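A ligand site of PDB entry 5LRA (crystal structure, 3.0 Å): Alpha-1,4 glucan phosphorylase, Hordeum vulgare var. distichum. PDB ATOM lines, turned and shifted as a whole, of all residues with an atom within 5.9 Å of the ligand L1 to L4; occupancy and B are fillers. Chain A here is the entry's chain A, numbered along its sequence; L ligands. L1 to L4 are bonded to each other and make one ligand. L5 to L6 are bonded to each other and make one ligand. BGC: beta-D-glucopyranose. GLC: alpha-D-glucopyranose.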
ATOM      1  N   GLU A  93      32.559  12.663  22.137  1.00  0.00           N
ATOM      2  CA  GLU A  93      32.654  11.797  20.961  1.00  0.00           C
ATOM      3  C   GLU A  93      33.650  10.677  21.183  1.00  0.00           C
ATOM      4  O   GLU A  93      34.673  10.900  21.804  1.00  0.00           O
ATOM      5  CB  GLU A  93      33.158  12.594  19.766  1.00  0.00           C
ATOM      6  CG  GLU A  93      32.188  13.565  19.126  1.00  0.00           C
ATOM      7  CD  GLU A  93      32.756  14.146  17.839  1.00  0.00           C
ATOM      8  OE1 GLU A  93      33.163  13.380  16.944  1.00  0.00           O
ATOM      9  OE2 GLU A  93      32.797  15.384  17.723  1.00  0.00           O
ATOM     10  N   ASN A 138      31.351  11.458  15.580  1.00  0.00           N
ATOM     11  CA  ASN A 138      30.994  12.255  14.416  1.00  0.00           C
ATOM     12  C   ASN A 138      32.235  12.590  13.600  1.00  0.00           C
ATOM     13  O   ASN A 138      32.388  12.113  12.482  1.00  0.00           O
ATOM     14  CB  ASN A 138      30.276  13.528  14.893  1.00  0.00           C
ATOM     15  CG  ASN A 138      29.795  14.421  13.755  1.00  0.00           C
ATOM     16  OD1 ASN A 138      29.381  15.555  13.982  1.00  0.00           O
ATOM     17  ND2 ASN A 138      29.821  13.906  12.525  1.00  0.00           N
ATOM     18  N   GLY A 139      33.137  13.381  14.163  1.00  0.00           N
ATOM     19  CA  GLY A 139      34.294  13.874  13.413  1.00  0.00           C
ATOM     20  C   GLY A 139      35.636  13.500  14.008  1.00  0.00           C
ATOM     21  O   GLY A 139      35.742  12.523  14.768  1.00  0.00           O
ATOM     22  N   GLY A 140      36.651  14.293  13.652  1.00  0.00           N
ATOM     23  CA  GLY A 140      38.005  14.072  14.138  1.00  0.00           C
ATOM     24  C   GLY A 140      38.046  13.933  15.651  1.00  0.00           C
ATOM     25  O   GLY A 140      38.668  13.017  16.179  1.00  0.00           O
ATOM     26  N   LEU A 141      37.354  14.834  16.339  1.00  0.00           N
ATOM     27  CA  LEU A 141      37.345  14.868  17.799  1.00  0.00           C
ATOM     28  C   LEU A 141      37.144  13.510  18.413  1.00  0.00           C
ATOM     29  O   LEU A 141      37.730  13.183  19.444  1.00  0.00           O
ATOM     30  CB  LEU A 141      36.223  15.762  18.291  1.00  0.00           C
ATOM     31  CG  LEU A 141      36.471  16.396  19.650  1.00  0.00           C
ATOM     32  CD1 LEU A 141      37.007  17.796  19.451  1.00  0.00           C
ATOM     33  CD2 LEU A 141      35.195  16.420  20.478  1.00  0.00           C
ATOM     34  N   GLY A 142      36.266  12.718  17.780  1.00  0.00           N
ATOM     35  CA  GLY A 142      35.896  11.403  18.264  1.00  0.00           C
ATOM     36  C   GLY A 142      36.896  10.343  17.879  1.00  0.00           C
ATOM     37  O   GLY A 142      37.250   9.496  18.689  1.00  0.00           O
ATOM     38  N   LEU A 170      24.490  10.187  15.975  1.00  0.00           N
ATOM     39  CA  LEU A 170      24.171  11.427  15.307  1.00  0.00           C
ATOM     40  C   LEU A 170      23.071  11.166  14.274  1.00  0.00           C
ATOM     41  O   LEU A 170      21.973  11.718  14.392  1.00  0.00           O
ATOM     42  CB  LEU A 170      25.416  12.028  14.658  1.00  0.00           C
ATOM     43  CG  LEU A 170      25.193  13.398  13.996  1.00  0.00           C
ATOM     44  CD1 LEU A 170      24.892  14.472  15.040  1.00  0.00           C
ATOM     45  CD2 LEU A 170      26.405  13.758  13.150  1.00  0.00           C
ATOM     46  N   TYR A 287      25.161  15.512  19.932  1.00  0.00           N
ATOM     47  CA  TYR A 287      25.018  16.907  19.516  1.00  0.00           C
ATOM     48  C   TYR A 287      23.591  17.223  19.035  1.00  0.00           C
ATOM     49  O   TYR A 287      23.380  17.568  17.861  1.00  0.00           O
ATOM     50  CB  TYR A 287      26.027  17.217  18.390  1.00  0.00           C
ATOM     51  CG  TYR A 287      27.488  17.033  18.756  1.00  0.00           C
ATOM     52  CD1 TYR A 287      27.947  17.314  20.030  1.00  0.00           C
ATOM     53  CD2 TYR A 287      28.405  16.613  17.808  1.00  0.00           C
ATOM     54  CE1 TYR A 287      29.266  17.153  20.354  1.00  0.00           C
ATOM     55  CE2 TYR A 287      29.734  16.460  18.129  1.00  0.00           C
ATOM     56  CZ  TYR A 287      30.165  16.731  19.409  1.00  0.00           C
ATOM     57  OH  TYR A 287      31.479  16.584  19.782  1.00  0.00           O
ATOM     58  N   ASP A 290      19.887  22.463  18.942  1.00  0.00           N
ATOM     59  CA  ASP A 290      19.792  23.353  20.091  1.00  0.00           C
ATOM     60  C   ASP A 290      19.357  24.776  19.758  1.00  0.00           C
ATOM     61  O   ASP A 290      19.646  25.707  20.508  1.00  0.00           O
ATOM     62  CB  ASP A 290      21.154  23.408  20.807  1.00  0.00           C
ATOM     63  CG  ASP A 290      22.245  24.056  19.944  1.00  0.00           C
ATOM     64  OD1 ASP A 290      22.002  24.295  18.733  1.00  0.00           O
ATOM     65  OD2 ASP A 290      23.352  24.313  20.478  1.00  0.00           O
ATOM     66  N   GLU A 291      18.657  24.962  18.637  1.00  0.00           N
ATOM     67  CA  GLU A 291      18.079  26.259  18.332  1.00  0.00           C
ATOM     68  C   GLU A 291      16.886  26.541  19.236  1.00  0.00           C
ATOM     69  O   GLU A 291      16.334  27.629  19.216  1.00  0.00           O
ATOM     70  CB  GLU A 291      17.644  26.329  16.866  1.00  0.00           C
ATOM     71  CG  GLU A 291      18.803  26.545  15.914  1.00  0.00           C
ATOM     72  CD  GLU A 291      18.446  26.215  14.468  1.00  0.00           C
ATOM     73  OE1 GLU A 291      19.381  25.967  13.676  1.00  0.00           O
ATOM     74  OE2 GLU A 291      17.243  26.210  14.126  1.00  0.00           O
ATOM     75  N   ARG A 299      21.460  19.665  25.828  1.00  0.00           N
ATOM     76  CA  ARG A 299      22.866  19.738  25.456  1.00  0.00           C
ATOM     77  C   ARG A 299      23.697  19.921  26.723  1.00  0.00           C
ATOM     78  O   ARG A 299      24.758  19.337  26.867  1.00  0.00           O
ATOM     79  CB  ARG A 299      23.077  20.929  24.504  1.00  0.00           C
ATOM     80  CG  ARG A 299      24.343  20.910  23.683  1.00  0.00           C
ATOM     81  CD  ARG A 299      24.237  19.933  22.534  1.00  0.00           C
ATOM     82  NE  ARG A 299      23.884  20.553  21.247  1.00  0.00           N
ATOM     83  CZ  ARG A 299      24.733  20.848  20.244  1.00  0.00           C
ATOM     84  NH1 ARG A 299      26.033  20.612  20.361  1.00  0.00           N
ATOM     85  NH2 ARG A 299      24.293  21.374  19.117  1.00  0.00           N
ATOM     86  N   ASP A 341      37.990  19.743  24.102  1.00  0.00           N
ATOM     87  CA  ASP A 341      37.138  20.905  23.768  1.00  0.00           C
ATOM     88  C   ASP A 341      36.336  21.392  24.969  1.00  0.00           C
ATOM     89  O   ASP A 341      36.583  20.940  26.080  1.00  0.00           O
ATOM     90  CB  ASP A 341      36.256  20.623  22.560  1.00  0.00           C
ATOM     91  CG  ASP A 341      36.175  21.822  21.614  1.00  0.00           C
ATOM     92  OD1 ASP A 341      35.721  22.882  22.077  1.00  0.00           O
ATOM     93  OD2 ASP A 341      36.587  21.692  20.444  1.00  0.00           O
ATOM     94  N   HIS A 343      33.157  21.093  25.899  1.00  0.00           N
ATOM     95  CA  HIS A 343      31.990  20.358  26.383  1.00  0.00           C
ATOM     96  C   HIS A 343      32.121  19.951  27.868  1.00  0.00           C
ATOM     97  O   HIS A 343      31.172  20.147  28.637  1.00  0.00           O
ATOM     98  CB  HIS A 343      31.690  19.145  25.492  1.00  0.00           C
ATOM     99  CG  HIS A 343      31.629  19.467  24.015  1.00  0.00           C
ATOM    100  ND1 HIS A 343      32.596  19.042  23.126  1.00  0.00           N
ATOM    101  CD2 HIS A 343      30.722  20.157  23.296  1.00  0.00           C
ATOM    102  CE1 HIS A 343      32.275  19.461  21.908  1.00  0.00           C
ATOM    103  NE2 HIS A 343      31.142  20.138  21.990  1.00  0.00           N
ATOM    104  N   HIS A 379      40.168  22.486  20.023  1.00  0.00           N
ATOM    105  CA  HIS A 379      40.215  21.789  18.736  1.00  0.00           C
ATOM    106  C   HIS A 379      39.774  22.565  17.523  1.00  0.00           C
ATOM    107  O   HIS A 379      39.928  22.088  16.405  1.00  0.00           O
ATOM    108  CB  HIS A 379      39.340  20.552  18.803  1.00  0.00           C
ATOM    109  CG  HIS A 379      39.869  19.523  19.737  1.00  0.00           C
ATOM    110  ND1 HIS A 379      40.703  18.505  19.317  1.00  0.00           N
ATOM    111  CD2 HIS A 379      39.724  19.368  21.069  1.00  0.00           C
ATOM    112  CE1 HIS A 379      41.026  17.758  20.351  1.00  0.00           C
ATOM    113  NE2 HIS A 379      40.442  18.268  21.425  1.00  0.00           N
ATOM    114  N   THR A 380      39.184  23.733  17.718  1.00  0.00           N
ATOM    115  CA  THR A 380      38.825  24.571  16.589  1.00  0.00           C
ATOM    116  C   THR A 380      38.515  25.969  17.056  1.00  0.00           C
ATOM    117  O   THR A 380      37.741  26.182  17.999  1.00  0.00           O
ATOM    118  CB  THR A 380      37.639  24.036  15.719  1.00  0.00           C
ATOM    119  OG1 THR A 380      37.000  22.919  16.361  1.00  0.00           O
ATOM    120  CG2 THR A 380      38.130  23.624  14.314  1.00  0.00           C
ATOM    121  N   LEU A 382      36.615  27.573  15.435  1.00  0.00           N
ATOM    122  CA  LEU A 382      35.160  27.671  15.080  1.00  0.00           C
ATOM    123  C   LEU A 382      34.215  27.850  16.299  1.00  0.00           C
ATOM    124  O   LEU A 382      34.323  27.102  17.271  1.00  0.00           O
ATOM    125  CB  LEU A 382      34.709  26.425  14.300  1.00  0.00           C
ATOM    126  CG  LEU A 382      34.712  26.379  12.764  1.00  0.00           C
ATOM    127  CD1 LEU A 382      33.805  27.457  12.178  1.00  0.00           C
ATOM    128  CD2 LEU A 382      36.118  26.483  12.180  1.00  0.00           C
ATOM    129  N   GLU A 384      31.092  27.231  17.204  1.00  0.00           N
ATOM    130  CA  GLU A 384      30.203  26.166  17.689  1.00  0.00           C
ATOM    131  C   GLU A 384      30.898  25.368  18.802  1.00  0.00           C
ATOM    132  O   GLU A 384      30.251  24.632  19.572  1.00  0.00           O
ATOM    133  CB  GLU A 384      29.850  25.221  16.541  1.00  0.00           C
ATOM    134  CG  GLU A 384      29.500  25.905  15.218  1.00  0.00           C
ATOM    135  CD  GLU A 384      30.383  25.463  14.060  1.00  0.00           C
ATOM    136  OE1 GLU A 384      30.911  24.314  14.061  1.00  0.00           O
ATOM    137  OE2 GLU A 384      30.566  26.270  13.125  1.00  0.00           O
ATOM    138  N   ALA A 385      32.238  25.496  18.868  1.00  0.00           N
ATOM    139  CA  ALA A 385      33.076  24.884  19.902  1.00  0.00           C
ATOM    140  C   ALA A 385      33.397  25.867  21.046  1.00  0.00           C
ATOM    141  O   ALA A 385      33.595  25.416  22.180  1.00  0.00           O
ATOM    142  CB  ALA A 385      34.360  24.356  19.281  1.00  0.00           C
ATOM    143  N   ARG A 657      33.311  15.839   7.100  1.00  0.00           N
ATOM    144  CA  ARG A 657      32.103  16.574   7.487  1.00  0.00           C
ATOM    145  C   ARG A 657      31.797  17.674   6.467  1.00  0.00           C
ATOM    146  O   ARG A 657      32.691  18.414   6.068  1.00  0.00           O
ATOM    147  CB  ARG A 657      32.241  17.152   8.912  1.00  0.00           C
ATOM    148  CG  ARG A 657      32.680  16.140   9.980  1.00  0.00           C
ATOM    149  CD  ARG A 657      32.482  16.651  11.412  1.00  0.00           C
ATOM    150  NE  ARG A 657      33.326  17.812  11.748  1.00  0.00           N
ATOM    151  CZ  ARG A 657      32.941  19.097  11.687  1.00  0.00           C
ATOM    152  NH1 ARG A 657      33.806  20.055  12.028  1.00  0.00           N
ATOM    153  NH2 ARG A 657      31.713  19.443  11.315  1.00  0.00           N
ATOM    154  N   ILE A 658      30.547  17.777   6.042  1.00  0.00           N
ATOM    155  CA  ILE A 658      30.173  18.657   4.942  1.00  0.00           C
ATOM    156  C   ILE A 658      29.934  20.078   5.452  1.00  0.00           C
ATOM    157  O   ILE A 658      28.900  20.368   6.044  1.00  0.00           O
ATOM    158  CB  ILE A 658      28.904  18.159   4.216  1.00  0.00           C
ATOM    159  CG1 ILE A 658      29.070  16.709   3.754  1.00  0.00           C
ATOM    160  CG2 ILE A 658      28.563  19.072   3.038  1.00  0.00           C
ATOM    161  CD1 ILE A 658      30.213  16.483   2.771  1.00  0.00           C
ATOM    162  N   HIS A 659      30.903  20.949   5.225  1.00  0.00           N
ATOM    163  CA  HIS A 659      30.878  22.280   5.802  1.00  0.00           C
ATOM    164  C   HIS A 659      31.294  23.249   4.722  1.00  0.00           C
ATOM    165  O   HIS A 659      32.162  22.931   3.897  1.00  0.00           O
ATOM    166  CB  HIS A 659      31.853  22.338   6.987  1.00  0.00           C
ATOM    167  CG  HIS A 659      31.434  23.245   8.094  1.00  0.00           C
ATOM    168  ND1 HIS A 659      31.215  24.601   7.919  1.00  0.00           N
ATOM    169  CD2 HIS A 659      31.239  23.010   9.422  1.00  0.00           C
ATOM    170  CE1 HIS A 659      30.883  25.143   9.072  1.00  0.00           C
ATOM    171  NE2 HIS A 659      30.886  24.203  10.001  1.00  0.00           N
ATOM    172  N   GLU A 660      30.694  24.429   4.718  1.00  0.00           N
ATOM    173  CA  GLU A 660      31.069  25.456   3.763  1.00  0.00           C
ATOM    174  C   GLU A 660      32.594  25.653   3.792  1.00  0.00           C
ATOM    175  O   GLU A 660      33.198  25.834   2.735  1.00  0.00           O
ATOM    176  CB  GLU A 660      30.339  26.768   4.072  1.00  0.00           C
ATOM    177  CG  GLU A 660      28.837  26.742   3.759  1.00  0.00           C
ATOM    178  CD  GLU A 660      28.093  27.982   4.248  1.00  0.00           C
ATOM    179  OE1 GLU A 660      28.232  28.343   5.442  1.00  0.00           O
ATOM    180  OE2 GLU A 660      27.352  28.579   3.444  1.00  0.00           O
ATOM    181  N   TYR A 661      33.184  25.579   4.985  1.00  0.00           N
ATOM    182  CA  TYR A 661      34.613  25.896   5.178  1.00  0.00           C
ATOM    183  C   TYR A 661      35.577  24.801   4.741  1.00  0.00           C
ATOM    184  O   TYR A 661      36.731  25.090   4.425  1.00  0.00           O
ATOM    185  CB  TYR A 661      34.883  26.301   6.650  1.00  0.00           C
ATOM    186  CG  TYR A 661      35.401  25.226   7.611  1.00  0.00           C
ATOM    187  CD1 TYR A 661      36.746  24.865   7.653  1.00  0.00           C
ATOM    188  CD2 TYR A 661      34.534  24.624   8.531  1.00  0.00           C
ATOM    189  CE1 TYR A 661      37.212  23.909   8.544  1.00  0.00           C
ATOM    190  CE2 TYR A 661      35.000  23.668   9.422  1.00  0.00           C
ATOM    191  CZ  TYR A 661      36.332  23.319   9.427  1.00  0.00           C
ATOM    192  OH  TYR A 661      36.783  22.376  10.302  1.00  0.00           O
ATOM    193  N   PHE A 702      25.488  18.343   8.841  1.00  0.00           N
ATOM    194  CA  PHE A 702      24.670  18.533  10.045  1.00  0.00           C
ATOM    195  C   PHE A 702      23.256  18.861   9.574  1.00  0.00           C
ATOM    196  O   PHE A 702      23.060  19.700   8.690  1.00  0.00           O
ATOM    197  CB  PHE A 702      25.243  19.612  10.997  1.00  0.00           C
ATOM    198  CG  PHE A 702      24.660  19.559  12.396  1.00  0.00           C
ATOM    199  CD1 PHE A 702      25.145  18.651  13.346  1.00  0.00           C
ATOM    200  CD2 PHE A 702      23.632  20.428  12.777  1.00  0.00           C
ATOM    201  CE1 PHE A 702      24.607  18.598  14.627  1.00  0.00           C
ATOM    202  CE2 PHE A 702      23.094  20.389  14.063  1.00  0.00           C
ATOM    203  CZ  PHE A 702      23.588  19.473  14.991  1.00  0.00           C
ATOM    204  N   THR A 704      20.504  20.266  10.356  1.00  0.00           N
ATOM    205  CA  THR A 704      19.843  21.560  10.438  1.00  0.00           C
ATOM    206  C   THR A 704      20.551  22.619   9.557  1.00  0.00           C
ATOM    207  O   THR A 704      19.941  23.604   9.115  1.00  0.00           O
ATOM    208  CB  THR A 704      19.732  21.967  11.940  1.00  0.00           C
ATOM    209  OG1 THR A 704      18.555  22.761  12.141  1.00  0.00           O
ATOM    210  CG2 THR A 704      20.979  22.697  12.449  1.00  0.00           C
ATOM    211  N   TYR A 705      21.838  22.371   9.268  1.00  0.00           N
ATOM    212  CA  TYR A 705      22.686  23.182   8.391  1.00  0.00           C
ATOM    213  C   TYR A 705      22.166  23.133   6.951  1.00  0.00           C
ATOM    214  O   TYR A 705      22.530  22.253   6.162  1.00  0.00           O
ATOM    215  CB  TYR A 705      24.131  22.646   8.465  1.00  0.00           C
ATOM    216  CG  TYR A 705      25.272  23.561   8.048  1.00  0.00           C
ATOM    217  CD1 TYR A 705      25.082  24.625   7.157  1.00  0.00           C
ATOM    218  CD2 TYR A 705      26.563  23.313   8.506  1.00  0.00           C
ATOM    219  CE1 TYR A 705      26.139  25.422   6.764  1.00  0.00           C
ATOM    220  CE2 TYR A 705      27.632  24.107   8.119  1.00  0.00           C
ATOM    221  CZ  TYR A 705      27.412  25.163   7.256  1.00  0.00           C
ATOM    222  OH  TYR A 705      28.469  25.973   6.868  1.00  0.00           O
ATOM    223  N   VAL A 706      21.316  24.102   6.615  1.00  0.00           N
ATOM    224  CA  VAL A 706      20.593  24.112   5.346  1.00  0.00           C
ATOM    225  C   VAL A 706      21.501  24.138   4.138  1.00  0.00           C
ATOM    226  O   VAL A 706      21.277  23.382   3.184  1.00  0.00           O
ATOM    227  CB  VAL A 706      19.659  25.334   5.245  1.00  0.00           C
ATOM    228  CG1 VAL A 706      19.015  25.396   3.858  1.00  0.00           C
ATOM    229  CG2 VAL A 706      18.619  25.295   6.359  1.00  0.00           C
ATOM    230  N   TYR A 858      25.500  38.239   5.563  1.00  0.00           N
ATOM    231  CA  TYR A 858      25.541  36.873   6.075  1.00  0.00           C
ATOM    232  C   TYR A 858      25.073  35.859   5.034  1.00  0.00           C
ATOM    233  O   TYR A 858      24.051  36.075   4.388  1.00  0.00           O
ATOM    234  CB  TYR A 858      24.656  36.743   7.333  1.00  0.00           C
ATOM    235  CG  TYR A 858      24.808  35.421   8.031  1.00  0.00           C
ATOM    236  CD1 TYR A 858      25.751  35.241   9.032  1.00  0.00           C
ATOM    237  CD2 TYR A 858      24.020  34.329   7.664  1.00  0.00           C
ATOM    238  CE1 TYR A 858      25.910  34.023   9.662  1.00  0.00           C
ATOM    239  CE2 TYR A 858      24.173  33.091   8.285  1.00  0.00           C
ATOM    240  CZ  TYR A 858      25.119  32.951   9.277  1.00  0.00           C
ATOM    241  OH  TYR A 858      25.269  31.738   9.892  1.00  0.00           O
ATOM    242  N   PHE A 864      34.149  32.055   2.461  1.00  0.00           N
ATOM    243  CA  PHE A 864      35.194  31.035   2.507  1.00  0.00           C
ATOM    244  C   PHE A 864      36.100  31.018   1.272  1.00  0.00           C
ATOM    245  O   PHE A 864      36.799  30.024   1.036  1.00  0.00           O
ATOM    246  CB  PHE A 864      34.563  29.690   2.745  1.00  0.00           C
ATOM    247  CG  PHE A 864      33.782  29.631   4.006  1.00  0.00           C
ATOM    248  CD1 PHE A 864      34.399  29.334   5.202  1.00  0.00           C
ATOM    249  CD2 PHE A 864      32.429  29.913   4.005  1.00  0.00           C
ATOM    250  CE1 PHE A 864      33.674  29.286   6.379  1.00  0.00           C
ATOM    251  CE2 PHE A 864      31.697  29.860   5.177  1.00  0.00           C
ATOM    252  CZ  PHE A 864      32.327  29.547   6.374  1.00  0.00           C
HETATM  253  C2  BGC L   1      24.197  27.709  10.302  1.00  0.00           C
HETATM  254  C3  BGC L   1      24.508  26.686  11.407  1.00  0.00           C
HETATM  255  C4  BGC L   1      25.893  26.065  11.238  1.00  0.00           C
HETATM  256  C5  BGC L   1      26.923  27.176  10.976  1.00  0.00           C
HETATM  257  C6  BGC L   1      28.346  26.641  10.841  1.00  0.00           C
HETATM  258  C1  BGC L   1      25.376  28.607   9.933  1.00  0.00           C
HETATM  259  O1  BGC L   1      25.114  29.295   8.713  1.00  0.00           O
HETATM  260  O2  BGC L   1      23.107  28.517  10.713  1.00  0.00           O
HETATM  261  O3  BGC L   1      23.502  25.710  11.385  1.00  0.00           O
HETATM  262  O4  BGC L   1      26.285  25.280  12.365  1.00  0.00           O
HETATM  263  O5  BGC L   1      26.566  27.855   9.787  1.00  0.00           O
HETATM  264  O6  BGC L   1      29.239  27.651  10.433  1.00  0.00           O
HETATM  265  C1  GLC L   2      25.719  23.941  12.393  1.00  0.00           C
HETATM  266  C2  GLC L   2      24.927  23.695  13.684  1.00  0.00           C
HETATM  267  C3  GLC L   2      25.843  23.422  14.887  1.00  0.00           C
HETATM  268  C4  GLC L   2      26.807  22.286  14.553  1.00  0.00           C
HETATM  269  C5  GLC L   2      27.568  22.598  13.267  1.00  0.00           C
HETATM  270  C6  GLC L   2      28.484  21.433  12.912  1.00  0.00           C
HETATM  271  O2  GLC L   2      24.048  24.774  13.914  1.00  0.00           O
HETATM  272  O3  GLC L   2      25.129  23.113  16.070  1.00  0.00           O
HETATM  273  O4  GLC L   2      27.768  22.111  15.588  1.00  0.00           O
HETATM  274  O5  GLC L   2      26.684  22.910  12.197  1.00  0.00           O
HETATM  275  O6  GLC L   2      28.599  21.234  11.524  1.00  0.00           O
HETATM  276  C1  GLC L   3      27.745  20.806  16.192  1.00  0.00           C
HETATM  277  C2  GLC L   3      28.311  20.979  17.590  1.00  0.00           C
HETATM  278  C3  GLC L   3      29.802  21.192  17.526  1.00  0.00           C
HETATM  279  C4  GLC L   3      30.411  19.922  16.948  1.00  0.00           C
HETATM  280  C5  GLC L   3      29.855  19.731  15.537  1.00  0.00           C
HETATM  281  C6  GLC L   3      30.253  18.379  14.944  1.00  0.00           C
HETATM  282  O2  GLC L   3      27.700  22.114  18.148  1.00  0.00           O
HETATM  283  O3  GLC L   3      30.326  21.472  18.797  1.00  0.00           O
HETATM  284  O4  GLC L   3      31.806  20.119  16.865  1.00  0.00           O
HETATM  285  O5  GLC L   3      28.440  19.813  15.465  1.00  0.00           O
HETATM  286  O6  GLC L   3      29.594  18.224  13.702  1.00  0.00           O
HETATM  287  C1  GLC L   4      32.611  19.165  17.578  1.00  0.00           C
HETATM  288  C2  GLC L   4      33.813  19.906  18.172  1.00  0.00           C
HETATM  289  C3  GLC L   4      34.824  20.300  17.107  1.00  0.00           C
HETATM  290  C4  GLC L   4      35.237  19.081  16.284  1.00  0.00           C
HETATM  291  C5  GLC L   4      33.982  18.392  15.737  1.00  0.00           C
HETATM  292  C6  GLC L   4      34.306  17.126  14.924  1.00  0.00           C
HETATM  293  O2  GLC L   4      33.359  21.077  18.844  1.00  0.00           O
HETATM  294  O3  GLC L   4      35.937  20.930  17.703  1.00  0.00           O
HETATM  295  O4  GLC L   4      36.096  19.496  15.231  1.00  0.00           O
HETATM  296  O5  GLC L   4      33.050  18.083  16.764  1.00  0.00           O
HETATM  297  O6  GLC L   4      34.318  15.958  15.704  1.00  0.00           O
HETATM  298  C1  GLC L   5      29.156  38.841  10.178  1.00  0.00           C
HETATM  299  C2  GLC L   5      29.063  38.833   8.640  1.00  0.00           C
HETATM  300  C3  GLC L   5      29.072  37.401   8.081  1.00  0.00           C
HETATM  301  C4  GLC L   5      30.020  36.420   8.800  1.00  0.00           C
HETATM  302  C5  GLC L   5      30.430  36.868  10.205  1.00  0.00           C
HETATM  303  C6  GLC L   5      31.825  36.357  10.552  1.00  0.00           C
HETATM  304  O1  GLC L   5      27.830  38.464  10.496  1.00  0.00           O
HETATM  305  O2  GLC L   5      27.918  39.551   8.194  1.00  0.00           O
HETATM  306  O3  GLC L   5      29.461  37.453   6.712  1.00  0.00           O
HETATM  307  O4  GLC L   5      29.403  35.154   8.930  1.00  0.00           O
HETATM  308  O5  GLC L   5      30.447  38.289  10.308  1.00  0.00           O
HETATM  309  O6  GLC L   5      32.219  37.002  11.731  1.00  0.00           O
HETATM  310  C1  GLC L   6      30.115  34.135   8.192  1.00  0.00           C
HETATM  311  C2  GLC L   6      29.595  34.032   6.734  1.00  0.00           C
HETATM  312  C3  GLC L   6      28.593  32.902   6.445  1.00  0.00           C
HETATM  313  C4  GLC L   6      28.969  31.640   7.205  1.00  0.00           C
HETATM  314  C5  GLC L   6      29.129  31.944   8.695  1.00  0.00           C
HETATM  315  C6  GLC L   6      29.455  30.687   9.514  1.00  0.00           C
HETATM  316  O2  GLC L   6      29.030  35.246   6.270  1.00  0.00           O
HETATM  317  O3  GLC L   6      28.510  32.658   5.047  1.00  0.00           O
HETATM  318  O4  GLC L   6      27.979  30.644   6.988  1.00  0.00           O
HETATM  319  O5  GLC L   6      30.152  32.902   8.895  1.00  0.00           O
HETATM  320  O6  GLC L   6      29.045  29.488   8.886  1.00  0.00           O
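The side-chain carboxylate of Glu 93 lies within hydrogen-bond range of an oxygen (O6) of GLC L4, at 2.6 Å. O3 of GLC L4 lies within hydrogen-bond range of OG1 of Thr 380, at 2.6 Å. OD1 of Asn 138 sits at hydrogen-bond distance from O6 of GLC L3. O1 of BGC L1 is in hydrogen-bond range of OH of Tyr 858 (2.7 Å). An oxygen (O3) of GLC L4 is in hydrogen-bond range of the side-chain carboxylate of Asp 341. An oxygen (O6) of GLC L4 lies close to the backbone NH (N) of Gly 139 (3.2 Å). NH1 of Arg 299 sits at hydrogen-bond distance from O2 of GLC L3. The backbone carbonyl oxygen (O) of Glu 384 is in hydrogen-bond range of an oxygen (O3) of GLC L3 (3.3 Å). An oxygen (O6) of BGC L1 sits close to the side-chain carboxylate of Glu 384 (3.3 Å). The backbone NH (N) of Leu 141 lies close to an oxygen (O6) of GLC L4, at 3.3 Å. The guanidinium group of Arg 657 is in hydrogen-bond range of an oxygen (O6) of GLC L3 (3.4 Å). An oxygen (O4) of GLC L6 is in hydrogen-bond range of the side-chain carboxylate (OE1) of Glu 660.
O6 of BGC L1 sits at hydrogen-bond distance from O6 of GLC L6, at 2.4 Å.
OE1 of Glu 93 is in hydrogen-bond range of N of Asn 138 (3.0 Å). The side-chain carboxylate of Glu 93 sits at hydrogen-bond distance from the backbone NH of Gly 139 (2.8 Å). The side-chain hydroxyl (OH) of Tyr 287 is in hydrogen-bond range of the side-chain carboxylate (OE2) of Glu 93, 2.7 Å away. The side-chain carboxylate (OE1) of Glu 93 is in hydrogen-bond range of the backbone NH (N) of Gly 142 (3.3 Å). The side-chain carboxylate of Asp 290 is in salt-bridge range of the guanidinium group of Arg 299. A ring nitrogen (ND1) of His 659 lies within hydrogen-bond range of the side-chain hydroxyl (OH) of Tyr 705. OH of Tyr 705 sits at hydrogen-bond distance from OE1 of Glu 660, 2.8 Å away.
N of Gly 140 touches O6 of GLC L4, 3.5 Å away. OH of Tyr 287 touches C1 of GLC L4 (3.6 Å). NE2 of His 343 touches O3 of GLC L3 (3.6 Å). His 379 touches the ligand L1 to L4. Ala 385 touches the ligand L1 to L4. CE1 of His 659 touches O6 of BGC L1, at 3.3 Å. Phe 702 touches the ligand L1 to L4. CG2 of Thr 704 touches O2 of GLC L2, 3.98 Å away. Tyr 705 touches the ligand L1 to L4. Of the 29 residues printed, 19 come within 4 Å of the ligand L1 to L4.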
